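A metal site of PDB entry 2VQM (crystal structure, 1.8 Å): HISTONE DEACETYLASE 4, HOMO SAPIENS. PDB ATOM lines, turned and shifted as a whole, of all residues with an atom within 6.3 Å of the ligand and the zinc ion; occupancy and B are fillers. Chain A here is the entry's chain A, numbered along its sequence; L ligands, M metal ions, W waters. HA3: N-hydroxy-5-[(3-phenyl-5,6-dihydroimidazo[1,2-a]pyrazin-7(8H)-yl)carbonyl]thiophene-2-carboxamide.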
ATOM      1  N   ARG A  37     -15.898  -6.708  36.861  1.00  0.00           N
ATOM      2  CA  ARG A  37     -16.800  -7.614  36.128  1.00  0.00           C
ATOM      3  C   ARG A  37     -16.836  -9.028  36.726  1.00  0.00           C
ATOM      4  O   ARG A  37     -17.907  -9.491  37.130  1.00  0.00           O
ATOM      5  CB  ARG A  37     -16.389  -7.678  34.656  1.00  0.00           C
ATOM      6  CG  ARG A  37     -16.298  -6.332  33.964  1.00  0.00           C
ATOM      7  CD  ARG A  37     -15.290  -6.384  32.832  1.00  0.00           C
ATOM      8  NE  ARG A  37     -15.769  -7.236  31.769  1.00  0.00           N
ATOM      9  CZ  ARG A  37     -15.140  -8.285  31.228  1.00  0.00           C
ATOM     10  NH1 ARG A  37     -13.941  -8.674  31.601  1.00  0.00           N
ATOM     11  NH2 ARG A  37     -15.744  -8.927  30.246  1.00  0.00           N
ATOM     12  N   PRO A 156     -10.409 -10.610  28.333  1.00  0.00           N
ATOM     13  CA  PRO A 156     -10.765 -11.452  27.173  1.00  0.00           C
ATOM     14  C   PRO A 156      -9.557 -11.862  26.353  1.00  0.00           C
ATOM     15  O   PRO A 156      -8.466 -11.284  26.496  1.00  0.00           O
ATOM     16  CB  PRO A 156     -11.699 -10.546  26.345  1.00  0.00           C
ATOM     17  CG  PRO A 156     -11.515  -9.199  26.854  1.00  0.00           C
ATOM     18  CD  PRO A 156     -10.956  -9.255  28.229  1.00  0.00           C
ATOM     19  N   HIS A 158      -9.998 -13.228  22.686  1.00  0.00           N
ATOM     20  CA  HIS A 158     -10.255 -13.554  21.275  1.00  0.00           C
ATOM     21  C   HIS A 158      -9.690 -12.603  20.197  1.00  0.00           C
ATOM     22  O   HIS A 158      -9.671 -12.973  19.001  1.00  0.00           O
ATOM     23  CB  HIS A 158     -11.764 -13.840  21.046  1.00  0.00           C
ATOM     24  CG  HIS A 158     -12.646 -12.631  21.096  1.00  0.00           C
ATOM     25  ND1 HIS A 158     -13.780 -12.505  20.322  1.00  0.00           N
ATOM     26  CD2 HIS A 158     -12.553 -11.493  21.823  1.00  0.00           C
ATOM     27  CE1 HIS A 158     -14.351 -11.345  20.575  1.00  0.00           C
ATOM     28  NE2 HIS A 158     -13.621 -10.708  21.477  1.00  0.00           N
ATOM     29  N   HIS A 159      -9.238 -11.411  20.591  1.00  0.00           N
ATOM     30  CA  HIS A 159      -8.588 -10.493  19.663  1.00  0.00           C
ATOM     31  C   HIS A 159      -7.067 -10.671  19.595  1.00  0.00           C
ATOM     32  O   HIS A 159      -6.438 -10.140  18.681  1.00  0.00           O
ATOM     33  CB  HIS A 159      -8.862  -9.025  20.009  1.00  0.00           C
ATOM     34  CG  HIS A 159     -10.302  -8.637  19.975  1.00  0.00           C
ATOM     35  ND1 HIS A 159     -11.107  -8.847  18.883  1.00  0.00           N
ATOM     36  CD2 HIS A 159     -11.077  -8.004  20.905  1.00  0.00           C
ATOM     37  CE1 HIS A 159     -12.324  -8.376  19.137  1.00  0.00           C
ATOM     38  NE2 HIS A 159     -12.324  -7.856  20.349  1.00  0.00           N
ATOM     39  N   MET A 166      -4.067  -6.993  21.370  1.00  0.00           N
ATOM     40  CA  MET A 166      -4.961  -5.902  20.940  1.00  0.00           C
ATOM     41  C   MET A 166      -6.335  -6.055  21.581  1.00  0.00           C
ATOM     42  O   MET A 166      -6.691  -7.127  22.085  1.00  0.00           O
ATOM     43  CB  MET A 166      -5.113  -5.845  19.414  1.00  0.00           C
ATOM     44  CG  MET A 166      -5.340  -7.180  18.729  1.00  0.00           C
ATOM     45  SD  MET A 166      -5.598  -7.065  16.942  1.00  0.00           S
ATOM     46  CE  MET A 166      -7.243  -6.380  16.910  1.00  0.00           C
ATOM     47  N   GLY A 167      -7.103  -4.960  21.544  1.00  0.00           N
ATOM     48  CA  GLY A 167      -8.449  -4.939  22.118  1.00  0.00           C
ATOM     49  C   GLY A 167      -8.566  -5.521  23.527  1.00  0.00           C
ATOM     50  O   GLY A 167      -9.521  -6.247  23.812  1.00  0.00           O
ATOM     51  N   PHE A 168      -7.595  -5.188  24.383  1.00  0.00           N
ATOM     52  CA  PHE A 168      -7.517  -5.602  25.794  1.00  0.00           C
ATOM     53  C   PHE A 168      -7.093  -7.076  25.980  1.00  0.00           C
ATOM     54  O   PHE A 168      -6.969  -7.557  27.122  1.00  0.00           O
ATOM     55  CB  PHE A 168      -8.821  -5.300  26.568  1.00  0.00           C
ATOM     56  CG  PHE A 168      -9.259  -3.866  26.458  1.00  0.00           C
ATOM     57  CD1 PHE A 168     -10.304  -3.501  25.617  1.00  0.00           C
ATOM     58  CD2 PHE A 168      -8.595  -2.883  27.156  1.00  0.00           C
ATOM     59  CE1 PHE A 168     -10.691  -2.171  25.491  1.00  0.00           C
ATOM     60  CE2 PHE A 168      -8.988  -1.541  27.035  1.00  0.00           C
ATOM     61  CZ  PHE A 168     -10.037  -1.197  26.201  1.00  0.00           C
ATOM     62  N   CYS A 169      -6.813  -7.774  24.882  1.00  0.00           N
ATOM     63  CA  CYS A 169      -6.439  -9.193  24.918  1.00  0.00           C
ATOM     64  C   CYS A 169      -4.914  -9.392  24.772  1.00  0.00           C
ATOM     65  O   CYS A 169      -4.297  -8.834  23.879  1.00  0.00           O
ATOM     66  CB  CYS A 169      -7.115  -9.953  23.769  1.00  0.00           C
ATOM     67  SG  CYS A 169      -8.895  -9.799  23.715  1.00  0.00           S
ATOM     68  N   ASP A 196     -19.560 -12.956  21.228  1.00  0.00           N
ATOM     69  CA  ASP A 196     -19.208 -11.597  21.584  1.00  0.00           C
ATOM     70  C   ASP A 196     -19.613 -10.707  20.366  1.00  0.00           C
ATOM     71  O   ASP A 196     -19.526 -11.157  19.224  1.00  0.00           O
ATOM     72  CB  ASP A 196     -17.705 -11.558  21.824  1.00  0.00           C
ATOM     73  CG  ASP A 196     -17.219 -10.218  22.324  1.00  0.00           C
ATOM     74  OD1 ASP A 196     -16.918 -10.118  23.544  1.00  0.00           O
ATOM     75  OD2 ASP A 196     -17.124  -9.293  21.492  1.00  0.00           O
ATOM     76  N   VAL A 197     -20.068  -9.479  20.608  1.00  0.00           N
ATOM     77  CA  VAL A 197     -20.481  -8.591  19.497  1.00  0.00           C
ATOM     78  C   VAL A 197     -19.331  -8.216  18.512  1.00  0.00           C
ATOM     79  O   VAL A 197     -19.589  -7.803  17.366  1.00  0.00           O
ATOM     80  CB  VAL A 197     -21.201  -7.325  20.059  1.00  0.00           C
ATOM     81  CG1 VAL A 197     -20.188  -6.331  20.622  1.00  0.00           C
ATOM     82  CG2 VAL A 197     -22.106  -6.702  18.971  1.00  0.00           C
ATOM     83  N   HIS A 198     -18.076  -8.389  18.949  1.00  0.00           N
ATOM     84  CA  HIS A 198     -16.897  -8.130  18.121  1.00  0.00           C
ATOM     85  C   HIS A 198     -16.340  -9.398  17.470  1.00  0.00           C
ATOM     86  O   HIS A 198     -16.359 -10.482  18.083  1.00  0.00           O
ATOM     87  CB  HIS A 198     -15.814  -7.454  18.975  1.00  0.00           C
ATOM     88  CG  HIS A 198     -16.282  -6.198  19.638  1.00  0.00           C
ATOM     89  ND1 HIS A 198     -16.604  -6.142  20.969  1.00  0.00           N
ATOM     90  CD2 HIS A 198     -16.482  -4.951  19.147  1.00  0.00           C
ATOM     91  CE1 HIS A 198     -17.009  -4.919  21.267  1.00  0.00           C
ATOM     92  NE2 HIS A 198     -16.933  -4.178  20.183  1.00  0.00           N
ATOM     93  N   PHE A 226     -16.646  -1.394  12.146  1.00  0.00           N
ATOM     94  CA  PHE A 226     -16.846  -1.637  13.588  1.00  0.00           C
ATOM     95  C   PHE A 226     -15.626  -2.414  14.127  1.00  0.00           C
ATOM     96  O   PHE A 226     -15.130  -3.305  13.447  1.00  0.00           O
ATOM     97  CB  PHE A 226     -18.155  -2.429  13.801  1.00  0.00           C
ATOM     98  CG  PHE A 226     -18.617  -2.447  15.226  1.00  0.00           C
ATOM     99  CD1 PHE A 226     -19.059  -1.283  15.841  1.00  0.00           C
ATOM    100  CD2 PHE A 226     -18.574  -3.615  15.969  1.00  0.00           C
ATOM    101  CE1 PHE A 226     -19.447  -1.280  17.177  1.00  0.00           C
ATOM    102  CE2 PHE A 226     -18.976  -3.631  17.298  1.00  0.00           C
ATOM    103  CZ  PHE A 226     -19.403  -2.475  17.908  1.00  0.00           C
ATOM    104  N   PHE A 227     -15.144  -2.074  15.321  1.00  0.00           N
ATOM    105  CA  PHE A 227     -13.987  -2.773  15.904  1.00  0.00           C
ATOM    106  C   PHE A 227     -14.119  -4.311  15.865  1.00  0.00           C
ATOM    107  O   PHE A 227     -15.200  -4.848  16.208  1.00  0.00           O
ATOM    108  CB  PHE A 227     -13.753  -2.335  17.357  1.00  0.00           C
ATOM    109  CG  PHE A 227     -12.455  -2.839  17.944  1.00  0.00           C
ATOM    110  CD1 PHE A 227     -11.281  -2.100  17.787  1.00  0.00           C
ATOM    111  CD2 PHE A 227     -12.405  -4.042  18.625  1.00  0.00           C
ATOM    112  CE1 PHE A 227     -10.081  -2.554  18.303  1.00  0.00           C
ATOM    113  CE2 PHE A 227     -11.188  -4.513  19.140  1.00  0.00           C
ATOM    114  CZ  PHE A 227     -10.022  -3.748  18.972  1.00  0.00           C
ATOM    115  N   GLY A 288     -18.750 -13.629  25.001  1.00  0.00           N
ATOM    116  CA  GLY A 288     -18.887 -12.218  25.376  1.00  0.00           C
ATOM    117  C   GLY A 288     -20.351 -11.883  25.475  1.00  0.00           C
ATOM    118  O   GLY A 288     -21.188 -12.475  24.762  1.00  0.00           O
ATOM    119  N   ASP A 290     -21.344  -8.449  25.363  1.00  0.00           N
ATOM    120  CA  ASP A 290     -21.469  -7.062  24.904  1.00  0.00           C
ATOM    121  C   ASP A 290     -22.554  -6.827  23.819  1.00  0.00           C
ATOM    122  O   ASP A 290     -22.827  -5.676  23.478  1.00  0.00           O
ATOM    123  CB  ASP A 290     -20.108  -6.404  24.523  1.00  0.00           C
ATOM    124  CG  ASP A 290     -19.178  -7.308  23.691  1.00  0.00           C
ATOM    125  OD1 ASP A 290     -19.679  -8.343  23.198  1.00  0.00           O
ATOM    126  OD2 ASP A 290     -17.943  -7.002  23.540  1.00  0.00           O
ATOM    127  N   PRO A 298     -21.162   2.856  20.289  1.00  0.00           N
ATOM    128  CA  PRO A 298     -19.782   2.530  19.876  1.00  0.00           C
ATOM    129  C   PRO A 298     -19.213   1.210  20.471  1.00  0.00           C
ATOM    130  O   PRO A 298     -18.497   0.484  19.768  1.00  0.00           O
ATOM    131  CB  PRO A 298     -18.974   3.751  20.357  1.00  0.00           C
ATOM    132  CG  PRO A 298     -19.734   4.263  21.496  1.00  0.00           C
ATOM    133  CD  PRO A 298     -21.193   3.844  21.369  1.00  0.00           C
ATOM    134  N   LEU A 299     -19.545   0.901  21.726  1.00  0.00           N
ATOM    135  CA  LEU A 299     -19.136  -0.344  22.379  1.00  0.00           C
ATOM    136  C   LEU A 299     -19.880  -1.573  21.806  1.00  0.00           C
ATOM    137  O   LEU A 299     -19.250  -2.586  21.480  1.00  0.00           O
ATOM    138  CB  LEU A 299     -19.367  -0.256  23.902  1.00  0.00           C
ATOM    139  CG  LEU A 299     -18.933  -1.442  24.778  1.00  0.00           C
ATOM    140  CD1 LEU A 299     -17.507  -1.917  24.461  1.00  0.00           C
ATOM    141  CD2 LEU A 299     -19.065  -1.094  26.272  1.00  0.00           C
ATOM    142  N   GLU A 329     -15.749 -13.544  27.461  1.00  0.00           N
ATOM    143  CA  GLU A 329     -14.890 -12.646  26.671  1.00  0.00           C
ATOM    144  C   GLU A 329     -15.261 -11.213  27.064  1.00  0.00           C
ATOM    145  O   GLU A 329     -15.010 -10.810  28.208  1.00  0.00           O
ATOM    146  CB  GLU A 329     -15.031 -12.917  25.167  1.00  0.00           C
ATOM    147  CG  GLU A 329     -14.590 -14.325  24.727  1.00  0.00           C
ATOM    148  CD  GLU A 329     -13.099 -14.501  24.500  1.00  0.00           C
ATOM    149  OE1 GLU A 329     -12.296 -13.557  24.711  1.00  0.00           O
ATOM    150  OE2 GLU A 329     -12.741 -15.620  24.057  1.00  0.00           O
ATOM    151  N   GLY A 330     -15.880 -10.451  26.160  1.00  0.00           N
ATOM    152  CA  GLY A 330     -16.309  -9.075  26.463  1.00  0.00           C
ATOM    153  C   GLY A 330     -17.643  -8.971  27.172  1.00  0.00           C
ATOM    154  O   GLY A 330     -18.211  -9.971  27.605  1.00  0.00           O
ATOM    155  N   GLY A 331     -18.170  -7.743  27.258  1.00  0.00           N
ATOM    156  CA  GLY A 331     -19.285  -7.427  28.132  1.00  0.00           C
ATOM    157  C   GLY A 331     -18.787  -6.489  29.223  1.00  0.00           C
ATOM    158  O   GLY A 331     -17.715  -6.716  29.781  1.00  0.00           O
HETATM  159  CAA HA3 L   1     -11.656   5.976  22.489  1.00  0.00           C
HETATM  160  CAB HA3 L   1     -12.308   7.200  22.290  1.00  0.00           C
HETATM  161  CAC HA3 L   1     -13.654   7.228  21.929  1.00  0.00           C
HETATM  162  CAD HA3 L   1     -14.358   6.029  21.766  1.00  0.00           C
HETATM  163  CAE HA3 L   1     -13.709   4.815  21.961  1.00  0.00           C
HETATM  164  CAF HA3 L   1     -12.347   4.772  22.330  1.00  0.00           C
HETATM  165  CAG HA3 L   1     -11.665   3.561  22.509  1.00  0.00           C
HETATM  166  CAH HA3 L   1     -10.559   3.291  23.232  1.00  0.00           C
HETATM  167  NAI HA3 L   1     -10.228   1.999  23.094  1.00  0.00           N
HETATM  168  CAJ HA3 L   1     -11.079   1.382  22.279  1.00  0.00           C
HETATM  169  CAK HA3 L   1     -11.118  -0.106  21.808  1.00  0.00           C
HETATM  170  NAL HA3 L   1     -12.022   2.366  21.877  1.00  0.00           N
HETATM  171  CAM HA3 L   1     -13.130   2.067  20.968  1.00  0.00           C
HETATM  172  CAN HA3 L   1     -12.749   0.877  20.155  1.00  0.00           C
HETATM  173  NAO HA3 L   1     -12.387  -0.233  21.053  1.00  0.00           N
HETATM  174  CAP HA3 L   1     -13.301  -1.183  21.179  1.00  0.00           C
HETATM  175  OAQ HA3 L   1     -14.334  -1.095  20.505  1.00  0.00           O
HETATM  176  CAR HA3 L   1     -13.143  -2.441  21.968  1.00  0.00           C
HETATM  177  SAS HA3 L   1     -14.444  -3.287  22.580  1.00  0.00           S
HETATM  178  CAT HA3 L   1     -12.020  -3.149  22.081  1.00  0.00           C
HETATM  179  CAU HA3 L   1     -12.192  -4.322  22.737  1.00  0.00           C
HETATM  180  CAV HA3 L   1     -13.464  -4.543  23.088  1.00  0.00           C
HETATM  181  CAW HA3 L   1     -13.976  -5.768  23.831  1.00  0.00           C
HETATM  182  OAY HA3 L   1     -15.197  -5.970  23.872  1.00  0.00           O
HETATM  183  NAX HA3 L   1     -13.052  -6.556  24.386  1.00  0.00           N
HETATM  184  OAZ HA3 L   1     -13.440  -7.667  25.061  1.00  0.00           O
HETATM  185 ZN    ZN M   1     -16.458  -7.621  22.496  1.00  0.00          ZN
HETATM  186  O   HOH W   1     -14.552  -8.346  22.370  1.00  0.00           O
HETATM  187  O   HOH W   2     -17.081  -5.409  26.142  1.00  0.00           O
HETATM  188  O   HOH W   3     -16.700  -1.471  19.531  1.00  0.00           O
HETATM  189  O   HOH W   4      -8.039   0.823  23.473  1.00  0.00           O
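Of the 20 residues printed, 3 come within 4 Å of the zinc ion.
The nearest printed residue that does not touch the zinc ion is Gly 330 (4.2 Å).
OD1 of Asp 290 sits at hydrogen-bond distance from N of Val 197 (2.9 Å).
The backbone NH of Gly 330 is in hydrogen-bond range of the side-chain carboxylate of Asp 196.
A ring nitrogen (NE2) of His 198 lies within hydrogen-bond range of the backbone carbonyl oxygen (O) of Leu 299 (3.1 Å).
SG of Cys 169 is in hydrogen-bond range of O of Pro 156 (3.2 Å).
O of Gly 167 is in hydrogen-bond range of SG of Cys 169 (3.6 Å).
Merely in contact with the ligand: Pro 156, Gly 167, Phe 168, Phe 227, Leu 299 and Gly 330.
Hydrophobic or aromatic side chains that line the ligand: Pro 156, Phe 168, His 198, Phe 227 and Leu 299.
Of the 20 residues printed, 8 come within 4 Å of the ligand.
The nearest printed residue that does not touch the ligand is His 159 (4.3 Å).
The zinc ion is bound by the side-chain carboxylate (OD2) of Asp 290 (1.9 Å), water W1 (2.0 Å), the side-chain carboxylate (OD2) of Asp 196 (2.1 Å), a ring nitrogen (ND1) of His 198 (2.1 Å) and an oxygen (OAY) of the ligand (2.5 Å).
The zinc ion has five donor atoms within binding distance.
Slightly farther from the zinc ion lies the side-chain carboxylate (OD1) of Asp 196 (2.7 Å).
Water W1 lies within hydrogen-bond range of NE2 of His 158 (2.7 Å), OAZ of the ligand (3.0 Å), NE2 of His 159 (3.0 Å) and OD1 of Asp 196 (3.2 Å).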
